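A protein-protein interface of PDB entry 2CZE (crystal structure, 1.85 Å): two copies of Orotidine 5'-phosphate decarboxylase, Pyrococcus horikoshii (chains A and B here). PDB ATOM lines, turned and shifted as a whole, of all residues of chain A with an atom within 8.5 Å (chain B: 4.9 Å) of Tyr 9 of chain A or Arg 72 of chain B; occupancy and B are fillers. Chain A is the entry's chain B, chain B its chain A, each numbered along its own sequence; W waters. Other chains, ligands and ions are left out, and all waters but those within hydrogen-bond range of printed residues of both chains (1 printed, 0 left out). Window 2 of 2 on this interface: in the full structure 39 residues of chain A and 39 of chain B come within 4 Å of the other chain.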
ATOM      1  N   LEU A   6     -18.693  24.746 -20.449  1.00  0.00           N
ATOM      2  CA  LEU A   6     -17.436  24.271 -21.012  1.00  0.00           C
ATOM      3  C   LEU A   6     -16.296  25.257 -20.808  1.00  0.00           C
ATOM      4  O   LEU A   6     -15.834  25.893 -21.747  1.00  0.00           O
ATOM      5  CB  LEU A   6     -17.653  23.996 -22.504  1.00  0.00           C
ATOM      6  CG  LEU A   6     -16.900  22.864 -23.185  1.00  0.00           C
ATOM      7  CD1 LEU A   6     -16.922  21.595 -22.318  1.00  0.00           C
ATOM      8  CD2 LEU A   6     -17.564  22.612 -24.537  1.00  0.00           C
ATOM      9  N   ASP A   7     -15.834  25.357 -19.567  1.00  0.00           N
ATOM     10  CA  ASP A   7     -14.766  26.278 -19.208  1.00  0.00           C
ATOM     11  C   ASP A   7     -13.354  25.699 -19.242  1.00  0.00           C
ATOM     12  O   ASP A   7     -12.671  25.660 -18.233  1.00  0.00           O
ATOM     13  CB  ASP A   7     -15.054  26.860 -17.829  1.00  0.00           C
ATOM     14  CG  ASP A   7     -16.394  27.559 -17.774  1.00  0.00           C
ATOM     15  OD1 ASP A   7     -17.081  27.419 -16.747  1.00  0.00           O
ATOM     16  OD2 ASP A   7     -16.753  28.240 -18.767  1.00  0.00           O
ATOM     17  N   VAL A   8     -12.942  25.235 -20.412  1.00  0.00           N
ATOM     18  CA  VAL A   8     -11.601  24.720 -20.615  1.00  0.00           C
ATOM     19  C   VAL A   8     -11.064  25.634 -21.714  1.00  0.00           C
ATOM     20  O   VAL A   8     -11.845  26.238 -22.456  1.00  0.00           O
ATOM     21  CB  VAL A   8     -11.612  23.238 -21.070  1.00  0.00           C
ATOM     22  CG1 VAL A   8     -12.238  22.375 -19.973  1.00  0.00           C
ATOM     23  CG2 VAL A   8     -12.370  23.077 -22.372  1.00  0.00           C
ATOM     24  N   TYR A   9      -9.746  25.778 -21.796  1.00  0.00           N
ATOM     25  CA  TYR A   9      -9.146  26.651 -22.809  1.00  0.00           C
ATOM     26  C   TYR A   9      -9.063  25.998 -24.190  1.00  0.00           C
ATOM     27  O   TYR A   9      -9.190  26.677 -25.212  1.00  0.00           O
ATOM     28  CB  TYR A   9      -7.721  27.041 -22.410  1.00  0.00           C
ATOM     29  CG  TYR A   9      -7.565  27.819 -21.123  1.00  0.00           C
ATOM     30  CD1 TYR A   9      -6.650  27.404 -20.152  1.00  0.00           C
ATOM     31  CD2 TYR A   9      -8.279  28.998 -20.895  1.00  0.00           C
ATOM     32  CE1 TYR A   9      -6.445  28.139 -18.990  1.00  0.00           C
ATOM     33  CE2 TYR A   9      -8.078  29.745 -19.733  1.00  0.00           C
ATOM     34  CZ  TYR A   9      -7.156  29.306 -18.785  1.00  0.00           C
ATOM     35  OH  TYR A   9      -6.940  30.024 -17.635  1.00  0.00           O
ATOM     36  N   GLU A  10      -8.843  24.683 -24.205  1.00  0.00           N
ATOM     37  CA  GLU A  10      -8.652  23.920 -25.443  1.00  0.00           C
ATOM     38  C   GLU A  10      -9.910  23.554 -26.225  1.00  0.00           C
ATOM     39  O   GLU A  10     -10.784  22.843 -25.718  1.00  0.00           O
ATOM     40  CB  GLU A  10      -7.874  22.635 -25.143  1.00  0.00           C
ATOM     41  CG  GLU A  10      -6.588  22.822 -24.342  1.00  0.00           C
ATOM     42  CD  GLU A  10      -6.818  22.939 -22.832  1.00  0.00           C
ATOM     43  OE1 GLU A  10      -5.811  23.067 -22.100  1.00  0.00           O
ATOM     44  OE2 GLU A  10      -7.986  22.903 -22.370  1.00  0.00           O
ATOM     45  N   GLY A  11      -9.969  24.001 -27.478  1.00  0.00           N
ATOM     46  CA  GLY A  11     -11.130  23.739 -28.318  1.00  0.00           C
ATOM     47  C   GLY A  11     -11.424  22.287 -28.664  1.00  0.00           C
ATOM     48  O   GLY A  11     -12.573  21.851 -28.583  1.00  0.00           O
ATOM     49  N   GLU A  12     -10.410  21.531 -29.072  1.00  0.00           N
ATOM     50  CA  GLU A  12     -10.634  20.125 -29.415  1.00  0.00           C
ATOM     51  C   GLU A  12     -11.083  19.347 -28.191  1.00  0.00           C
ATOM     52  O   GLU A  12     -11.953  18.475 -28.276  1.00  0.00           O
ATOM     53  CB  GLU A  12      -9.367  19.507 -30.012  1.00  0.00           C
ATOM     54  CG  GLU A  12      -9.199  19.835 -31.486  1.00  0.00           C
ATOM     55  CD  GLU A  12     -10.379  19.347 -32.323  1.00  0.00           C
ATOM     56  OE1 GLU A  12     -10.724  18.148 -32.242  1.00  0.00           O
ATOM     57  OE2 GLU A  12     -10.967  20.161 -33.066  1.00  0.00           O
ATOM     58  N   ARG A  13     -10.497  19.684 -27.048  1.00  0.00           N
ATOM     59  CA  ARG A  13     -10.843  19.051 -25.788  1.00  0.00           C
ATOM     60  C   ARG A  13     -12.303  19.373 -25.443  1.00  0.00           C
ATOM     61  O   ARG A  13     -13.053  18.506 -24.998  1.00  0.00           O
ATOM     62  CB  ARG A  13      -9.924  19.575 -24.683  1.00  0.00           C
ATOM     63  CG  ARG A  13     -10.236  19.046 -23.299  1.00  0.00           C
ATOM     64  CD  ARG A  13      -9.422  19.784 -22.243  1.00  0.00           C
ATOM     65  NE  ARG A  13      -9.793  19.384 -20.889  1.00  0.00           N
ATOM     66  CZ  ARG A  13      -9.384  20.012 -19.792  1.00  0.00           C
ATOM     67  NH1 ARG A  13      -8.589  21.071 -19.895  1.00  0.00           N
ATOM     68  NH2 ARG A  13      -9.775  19.586 -18.595  1.00  0.00           N
ATOM     69  N   ALA A  14     -12.705  20.623 -25.657  1.00  0.00           N
ATOM     70  CA  ALA A  14     -14.067  21.038 -25.357  1.00  0.00           C
ATOM     71  C   ALA A  14     -15.070  20.291 -26.235  1.00  0.00           C
ATOM     72  O   ALA A  14     -16.104  19.817 -25.761  1.00  0.00           O
ATOM     73  CB  ALA A  14     -14.209  22.546 -25.559  1.00  0.00           C
ATOM     74  N   ASN A  31     -17.898  30.473 -22.059  1.00  0.00           N
ATOM     75  CA  ASN A  31     -17.550  31.673 -21.287  1.00  0.00           C
ATOM     76  C   ASN A  31     -16.233  32.191 -21.882  1.00  0.00           C
ATOM     77  O   ASN A  31     -15.702  31.609 -22.836  1.00  0.00           O
ATOM     78  CB  ASN A  31     -17.363  31.304 -19.805  1.00  0.00           C
ATOM     79  CG  ASN A  31     -17.573  32.464 -18.852  1.00  0.00           C
ATOM     80  OD1 ASN A  31     -17.153  33.587 -19.116  1.00  0.00           O
ATOM     81  ND2 ASN A  31     -18.199  32.183 -17.711  1.00  0.00           N
ATOM     82  N   TRP A  32     -15.692  33.262 -21.310  1.00  0.00           N
ATOM     83  CA  TRP A  32     -14.451  33.843 -21.815  1.00  0.00           C
ATOM     84  C   TRP A  32     -13.233  32.917 -21.877  1.00  0.00           C
ATOM     85  O   TRP A  32     -12.427  33.027 -22.793  1.00  0.00           O
ATOM     86  CB  TRP A  32     -14.095  35.101 -21.021  1.00  0.00           C
ATOM     87  CG  TRP A  32     -15.047  36.250 -21.254  1.00  0.00           C
ATOM     88  CD1 TRP A  32     -15.793  36.898 -20.307  1.00  0.00           C
ATOM     89  CD2 TRP A  32     -15.343  36.893 -22.507  1.00  0.00           C
ATOM     90  NE1 TRP A  32     -16.532  37.895 -20.890  1.00  0.00           N
ATOM     91  CE2 TRP A  32     -16.275  37.919 -22.235  1.00  0.00           C
ATOM     92  CE3 TRP A  32     -14.909  36.703 -23.830  1.00  0.00           C
ATOM     93  CZ2 TRP A  32     -16.784  38.755 -23.237  1.00  0.00           C
ATOM     94  CZ3 TRP A  32     -15.413  37.531 -24.825  1.00  0.00           C
ATOM     95  CH2 TRP A  32     -16.343  38.546 -24.522  1.00  0.00           C
ATOM     96  N   PRO A  33     -13.071  32.005 -20.900  1.00  0.00           N
ATOM     97  CA  PRO A  33     -11.903  31.105 -20.951  1.00  0.00           C
ATOM     98  C   PRO A  33     -11.771  30.341 -22.289  1.00  0.00           C
ATOM     99  O   PRO A  33     -10.707  30.331 -22.903  1.00  0.00           O
ATOM    100  CB  PRO A  33     -12.149  30.155 -19.776  1.00  0.00           C
ATOM    101  CG  PRO A  33     -12.879  31.048 -18.780  1.00  0.00           C
ATOM    102  CD  PRO A  33     -13.859  31.789 -19.676  1.00  0.00           C
ATOM    103  N   LEU A  34     -12.852  29.704 -22.736  1.00  0.00           N
ATOM    104  CA  LEU A  34     -12.822  28.946 -23.994  1.00  0.00           C
ATOM    105  C   LEU A  34     -12.696  29.879 -25.192  1.00  0.00           C
ATOM    106  O   LEU A  34     -11.943  29.591 -26.134  1.00  0.00           O
ATOM    107  CB  LEU A  34     -14.086  28.087 -24.143  1.00  0.00           C
ATOM    108  CG  LEU A  34     -14.193  27.172 -25.376  1.00  0.00           C
ATOM    109  CD1 LEU A  34     -12.977  26.257 -25.474  1.00  0.00           C
ATOM    110  CD2 LEU A  34     -15.469  26.344 -25.273  1.00  0.00           C
ATOM    111  N   ILE A  35     -13.407  31.006 -25.157  1.00  0.00           N
ATOM    112  CA  ILE A  35     -13.331  31.960 -26.264  1.00  0.00           C
ATOM    113  C   ILE A  35     -11.906  32.499 -26.418  1.00  0.00           C
ATOM    114  O   ILE A  35     -11.407  32.653 -27.541  1.00  0.00           O
ATOM    115  CB  ILE A  35     -14.340  33.130 -26.059  1.00  0.00           C
ATOM    116  CG1 ILE A  35     -15.765  32.589 -26.214  1.00  0.00           C
ATOM    117  CG2 ILE A  35     -14.063  34.269 -27.040  1.00  0.00           C
ATOM    118  CD1 ILE A  35     -16.866  33.576 -25.864  1.00  0.00           C
ATOM    119  N   LEU A  36     -11.258  32.789 -25.291  1.00  0.00           N
ATOM    120  CA  LEU A  36      -9.884  33.295 -25.303  1.00  0.00           C
ATOM    121  C   LEU A  36      -8.929  32.209 -25.793  1.00  0.00           C
ATOM    122  O   LEU A  36      -8.057  32.445 -26.629  1.00  0.00           O
ATOM    123  CB  LEU A  36      -9.469  33.721 -23.896  1.00  0.00           C
ATOM    124  CG  LEU A  36     -10.022  35.066 -23.433  1.00  0.00           C
ATOM    125  CD1 LEU A  36      -9.881  35.220 -21.924  1.00  0.00           C
ATOM    126  CD2 LEU A  36      -9.295  36.170 -24.176  1.00  0.00           C
ATOM    127  N   GLY A  37      -9.128  31.002 -25.282  1.00  0.00           N
ATOM    128  CA  GLY A  37      -8.274  29.894 -25.653  1.00  0.00           C
ATOM    129  C   GLY A  37      -8.408  29.360 -27.064  1.00  0.00           C
ATOM    130  O   GLY A  37      -7.405  28.950 -27.652  1.00  0.00           O
ATOM    131  N   SER A  38      -9.620  29.370 -27.619  1.00  0.00           N
ATOM    132  CA  SER A  38      -9.834  28.812 -28.955  1.00  0.00           C
ATOM    133  C   SER A  38     -10.377  29.769 -30.008  1.00  0.00           C
ATOM    134  O   SER A  38     -10.477  29.408 -31.182  1.00  0.00           O
ATOM    135  CB  SER A  38     -10.768  27.599 -28.847  1.00  0.00           C
ATOM    136  OG  SER A  38     -10.226  26.640 -27.955  1.00  0.00           O
ATOM    137  N   GLY A  39     -10.726  30.982 -29.598  1.00  0.00           N
ATOM    138  CA  GLY A  39     -11.267  31.948 -30.542  1.00  0.00           C
ATOM    139  C   GLY A  39     -12.783  31.896 -30.532  1.00  0.00           C
ATOM    140  O   GLY A  39     -13.363  30.854 -30.239  1.00  0.00           O
ATOM    141  N   ILE A  42     -15.120  29.081 -31.962  1.00  0.00           N
ATOM    142  CA  ILE A  42     -15.391  27.830 -31.257  1.00  0.00           C
ATOM    143  C   ILE A  42     -16.898  27.631 -31.091  1.00  0.00           C
ATOM    144  O   ILE A  42     -17.380  26.506 -31.004  1.00  0.00           O
ATOM    145  CB  ILE A  42     -14.708  27.809 -29.862  1.00  0.00           C
ATOM    146  CG1 ILE A  42     -14.694  26.386 -29.299  1.00  0.00           C
ATOM    147  CG2 ILE A  42     -15.440  28.731 -28.887  1.00  0.00           C
ATOM    148  CD1 ILE A  42     -13.890  25.391 -30.132  1.00  0.00           C
ATOM    149  N   ARG A  45     -18.192  26.040 -34.205  1.00  0.00           N
ATOM    150  CA  ARG A  45     -17.694  24.668 -34.199  1.00  0.00           C
ATOM    151  C   ARG A  45     -18.501  23.740 -33.289  1.00  0.00           C
ATOM    152  O   ARG A  45     -18.838  22.619 -33.673  1.00  0.00           O
ATOM    153  CB  ARG A  45     -16.214  24.631 -33.784  1.00  0.00           C
ATOM    154  CG  ARG A  45     -15.243  25.169 -34.842  1.00  0.00           C
ATOM    155  CD  ARG A  45     -13.791  24.755 -34.546  1.00  0.00           C
ATOM    156  NE  ARG A  45     -13.186  25.500 -33.440  1.00  0.00           N
ATOM    157  CZ  ARG A  45     -12.649  26.718 -33.546  1.00  0.00           C
ATOM    158  NH1 ARG A  45     -12.130  27.310 -32.477  1.00  0.00           N
ATOM    159  NH2 ARG A  45     -12.620  27.344 -34.718  1.00  0.00           N
ATOM    160  N   TYR A 189     -16.707  18.496 -16.554  1.00  0.00           N
ATOM    161  CA  TYR A 189     -15.433  18.561 -17.258  1.00  0.00           C
ATOM    162  C   TYR A 189     -14.198  18.230 -16.428  1.00  0.00           C
ATOM    163  O   TYR A 189     -13.126  17.998 -16.989  1.00  0.00           O
ATOM    164  CB  TYR A 189     -15.275  19.909 -18.004  1.00  0.00           C
ATOM    165  CG  TYR A 189     -14.985  21.153 -17.179  1.00  0.00           C
ATOM    166  CD1 TYR A 189     -13.749  21.330 -16.543  1.00  0.00           C
ATOM    167  CD2 TYR A 189     -15.923  22.185 -17.098  1.00  0.00           C
ATOM    168  CE1 TYR A 189     -13.451  22.511 -15.851  1.00  0.00           C
ATOM    169  CE2 TYR A 189     -15.645  23.352 -16.417  1.00  0.00           C
ATOM    170  CZ  TYR A 189     -14.405  23.519 -15.792  1.00  0.00           C
ATOM    171  OH  TYR A 189     -14.150  24.692 -15.113  1.00  0.00           O
ATOM    172  N   ASN B  67     -13.056  34.150 -12.940  1.00  0.00           N
ATOM    173  CA  ASN B  67     -12.244  35.374 -13.018  1.00  0.00           C
ATOM    174  C   ASN B  67     -10.768  34.954 -13.042  1.00  0.00           C
ATOM    175  O   ASN B  67      -9.953  35.516 -13.780  1.00  0.00           O
ATOM    176  CB  ASN B  67     -12.501  36.285 -11.796  1.00  0.00           C
ATOM    177  CG  ASN B  67     -13.641  37.279 -12.022  1.00  0.00           C
ATOM    178  OD1 ASN B  67     -14.466  37.116 -12.937  1.00  0.00           O
ATOM    179  ND2 ASN B  67     -13.692  38.310 -11.187  1.00  0.00           N
ATOM    180  N   ARG B  68     -10.432  33.949 -12.240  1.00  0.00           N
ATOM    181  CA  ARG B  68      -9.066  33.455 -12.206  1.00  0.00           C
ATOM    182  C   ARG B  68      -8.679  32.894 -13.571  1.00  0.00           C
ATOM    183  O   ARG B  68      -7.632  33.244 -14.112  1.00  0.00           O
ATOM    184  CB  ARG B  68      -8.903  32.361 -11.136  1.00  0.00           C
ATOM    185  CG  ARG B  68      -7.470  31.807 -11.033  1.00  0.00           C
ATOM    186  CD  ARG B  68      -7.375  30.759  -9.926  1.00  0.00           C
ATOM    187  NE  ARG B  68      -8.220  29.602 -10.219  1.00  0.00           N
ATOM    188  CZ  ARG B  68      -7.911  28.681 -11.127  1.00  0.00           C
ATOM    189  NH1 ARG B  68      -6.777  28.780 -11.820  1.00  0.00           N
ATOM    190  NH2 ARG B  68      -8.742  27.677 -11.364  1.00  0.00           N
ATOM    191  N   LEU B  69      -9.513  32.016 -14.124  1.00  0.00           N
ATOM    192  CA  LEU B  69      -9.212  31.432 -15.436  1.00  0.00           C
ATOM    193  C   LEU B  69      -9.030  32.491 -16.516  1.00  0.00           C
ATOM    194  O   LEU B  69      -8.122  32.397 -17.350  1.00  0.00           O
ATOM    195  CB  LEU B  69     -10.321  30.464 -15.880  1.00  0.00           C
ATOM    196  CG  LEU B  69     -10.442  29.174 -15.056  1.00  0.00           C
ATOM    197  CD1 LEU B  69     -11.631  28.338 -15.546  1.00  0.00           C
ATOM    198  CD2 LEU B  69      -9.149  28.386 -15.164  1.00  0.00           C
ATOM    199  N   ILE B  70      -9.893  33.497 -16.505  1.00  0.00           N
ATOM    200  CA  ILE B  70      -9.796  34.550 -17.511  1.00  0.00           C
ATOM    201  C   ILE B  70      -8.542  35.411 -17.341  1.00  0.00           C
ATOM    202  O   ILE B  70      -7.751  35.581 -18.283  1.00  0.00           O
ATOM    203  CB  ILE B  70     -11.025  35.467 -17.462  1.00  0.00           C
ATOM    204  CG1 ILE B  70     -12.295  34.647 -17.749  1.00  0.00           C
ATOM    205  CG2 ILE B  70     -10.843  36.613 -18.487  1.00  0.00           C
ATOM    206  CD1 ILE B  70     -13.618  35.403 -17.496  1.00  0.00           C
ATOM    207  N   ALA B  71      -8.368  35.951 -16.137  1.00  0.00           N
ATOM    208  CA  ALA B  71      -7.229  36.813 -15.831  1.00  0.00           C
ATOM    209  C   ALA B  71      -5.882  36.148 -16.065  1.00  0.00           C
ATOM    210  O   ALA B  71      -4.947  36.782 -16.543  1.00  0.00           O
ATOM    211  CB  ALA B  71      -7.312  37.304 -14.392  1.00  0.00           C
ATOM    212  N   ARG B  72      -5.766  34.869 -15.737  1.00  0.00           N
ATOM    213  CA  ARG B  72      -4.479  34.229 -15.914  1.00  0.00           C
ATOM    214  C   ARG B  72      -4.119  34.185 -17.399  1.00  0.00           C
ATOM    215  O   ARG B  72      -2.962  34.375 -17.768  1.00  0.00           O
ATOM    216  CB  ARG B  72      -4.472  32.838 -15.259  1.00  0.00           C
ATOM    217  CG  ARG B  72      -4.631  31.654 -16.170  1.00  0.00           C
ATOM    218  CD  ARG B  72      -4.788  30.371 -15.342  1.00  0.00           C
ATOM    219  NE  ARG B  72      -3.546  29.905 -14.725  1.00  0.00           N
ATOM    220  CZ  ARG B  72      -2.823  28.883 -15.179  1.00  0.00           C
ATOM    221  NH1 ARG B  72      -3.217  28.221 -16.256  1.00  0.00           N
ATOM    222  NH2 ARG B  72      -1.709  28.518 -14.550  1.00  0.00           N
ATOM    223  N   LYS B  73      -5.122  34.004 -18.250  1.00  0.00           N
ATOM    224  CA  LYS B  73      -4.900  33.950 -19.690  1.00  0.00           C
ATOM    225  C   LYS B  73      -4.571  35.330 -20.265  1.00  0.00           C
ATOM    226  O   LYS B  73      -3.703  35.461 -21.141  1.00  0.00           O
ATOM    227  CB  LYS B  73      -6.143  33.386 -20.381  1.00  0.00           C
ATOM    228  CG  LYS B  73      -6.004  33.186 -21.870  1.00  0.00           C
ATOM    229  CD  LYS B  73      -5.011  32.088 -22.232  1.00  0.00           C
ATOM    230  CE  LYS B  73      -4.927  31.945 -23.748  1.00  0.00           C
ATOM    231  NZ  LYS B  73      -3.950  30.911 -24.179  1.00  0.00           N
ATOM    232  N   VAL B  74      -5.253  36.363 -19.769  1.00  0.00           N
ATOM    233  CA  VAL B  74      -5.034  37.717 -20.263  1.00  0.00           C
ATOM    234  C   VAL B  74      -3.726  38.324 -19.733  1.00  0.00           C
ATOM    235  O   VAL B  74      -2.995  38.970 -20.482  1.00  0.00           O
ATOM    236  CB  VAL B  74      -6.251  38.600 -19.930  1.00  0.00           C
ATOM    237  CG1 VAL B  74      -6.030  40.027 -20.411  1.00  0.00           C
ATOM    238  CG2 VAL B  74      -7.490  38.004 -20.597  1.00  0.00           C
ATOM    239  N   PHE B  75      -3.409  38.112 -18.460  1.00  0.00           N
ATOM    240  CA  PHE B  75      -2.141  38.634 -17.945  1.00  0.00           C
ATOM    241  C   PHE B  75      -1.054  37.855 -18.685  1.00  0.00           C
ATOM    242  O   PHE B  75      -0.020  38.409 -19.051  1.00  0.00           O
ATOM    243  CB  PHE B  75      -1.998  38.383 -16.440  1.00  0.00           C
ATOM    244  CG  PHE B  75      -2.700  39.394 -15.570  1.00  0.00           C
ATOM    245  CD1 PHE B  75      -2.410  40.745 -15.683  1.00  0.00           C
ATOM    246  CD2 PHE B  75      -3.611  38.983 -14.592  1.00  0.00           C
ATOM    247  CE1 PHE B  75      -3.014  41.684 -14.825  1.00  0.00           C
ATOM    248  CE2 PHE B  75      -4.215  39.902 -13.740  1.00  0.00           C
ATOM    249  CZ  PHE B  75      -3.914  41.259 -13.857  1.00  0.00           C
ATOM    250  N   GLY B  76      -1.312  36.572 -18.921  1.00  0.00           N
ATOM    251  CA  GLY B  76      -0.352  35.734 -19.621  1.00  0.00           C
ATOM    252  C   GLY B  76      -0.108  36.192 -21.044  1.00  0.00           C
ATOM    253  O   GLY B  76       0.933  35.898 -21.637  1.00  0.00           O
ATOM    254  N   LEU B  99      -3.206  37.659  -9.476  1.00  0.00           N
ATOM    255  CA  LEU B  99      -2.476  37.368 -10.717  1.00  0.00           C
ATOM    256  C   LEU B  99      -1.770  38.568 -11.358  1.00  0.00           C
ATOM    257  O   LEU B  99      -0.931  38.414 -12.245  1.00  0.00           O
ATOM    258  CB  LEU B  99      -3.446  36.755 -11.745  1.00  0.00           C
ATOM    259  CG  LEU B  99      -4.122  35.442 -11.328  1.00  0.00           C
ATOM    260  CD1 LEU B  99      -5.188  35.068 -12.360  1.00  0.00           C
ATOM    261  CD2 LEU B  99      -3.083  34.347 -11.214  1.00  0.00           C
HETATM  262  O   HOH W   1      -5.272  32.010 -26.871  1.00  0.00           O
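No position is printed for both chains. Of the 8 pairs that touch across the chains among the printed residues, none has its exchanged pair printed and touching as well.
Of chain B, only Leu 69 (2.7 Å) and Arg 72 (3.2 Å) come within 4 Å of Tyr 9 of chain A. Arg 72 of chain B touches just one residue of chain A: Tyr 9 (3.2 Å). No residue of chain A comes within 4 Å of Ala 71 of chain B. Printed residues of chain B within 4 Å of Trp 32 of chain A: Ile 70 (3.6 Å). Printed residues of chain A within 4 Å of Leu 69 of chain B: Asp 7 (3.9 Å), Tyr 9 (2.7 Å) and Pro 33 (3.9 Å). Asn 31 of chain A touches none of the printed residues of chain B. Ile 35 of chain A touches none of the printed residues of chain B. The nearest residue of chain A that does not touch Arg 72 of chain B is Leu 36 of chain A (7.4 Å). The nearest printed residue of chain B that does not touch Pro 33 of chain A is Lys 73 of chain B (5.6 Å).
Water W1 lies within hydrogen-bond range of the backbone carbonyl oxygen (O) of Leu 36 of chain A (2.8 Å) and the side-chain amino group (NZ) of Lys 73 of chain B (3.2 Å).
Of the 11 printed residues of chain B, 4 touch a printed residue of chain A. Hydrophobic or aromatic side chains of chain B within 4 Å of the printed part of chain A: Leu 69, Ile 70 and Val 74. Along chain B the printed residues that touch a printed residue of chain A span positions 69 to 74. Hydrophobic or aromatic side chains of chain A that line the printed part of chain B: Tyr 9, Trp 32, Pro 33 and Leu 36.
The backbone carbonyl oxygen of Tyr 9 of chain A lies within hydrogen-bond range of the side-chain hydroxyl of Ser 38 of chain A (2.9 Å).
CD1 of Leu 69 of chain B touches O of Asp 7 of chain A, 3.9 Å away. OH of Tyr 9 of chain A touches CD of Arg 72 of chain B (3.2 Å). CD1 of Ile 70 of chain B touches CB of Trp 32 of chain A (3.6 Å). Pro 33 of chain A touches Leu 69 of chain B. Ile 70 of chain B touches Pro 33 of chain A. CG2 of Ile 70 of chain B touches CD1 of Leu 36 of chain A (3.8 Å). Leu 36 of chain A touches Val 74 of chain B (CD1 to CG2, 3.9 Å).
OH of Tyr 9 of chain A is in hydrogen-bond range of O of Leu 69 of chain B.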
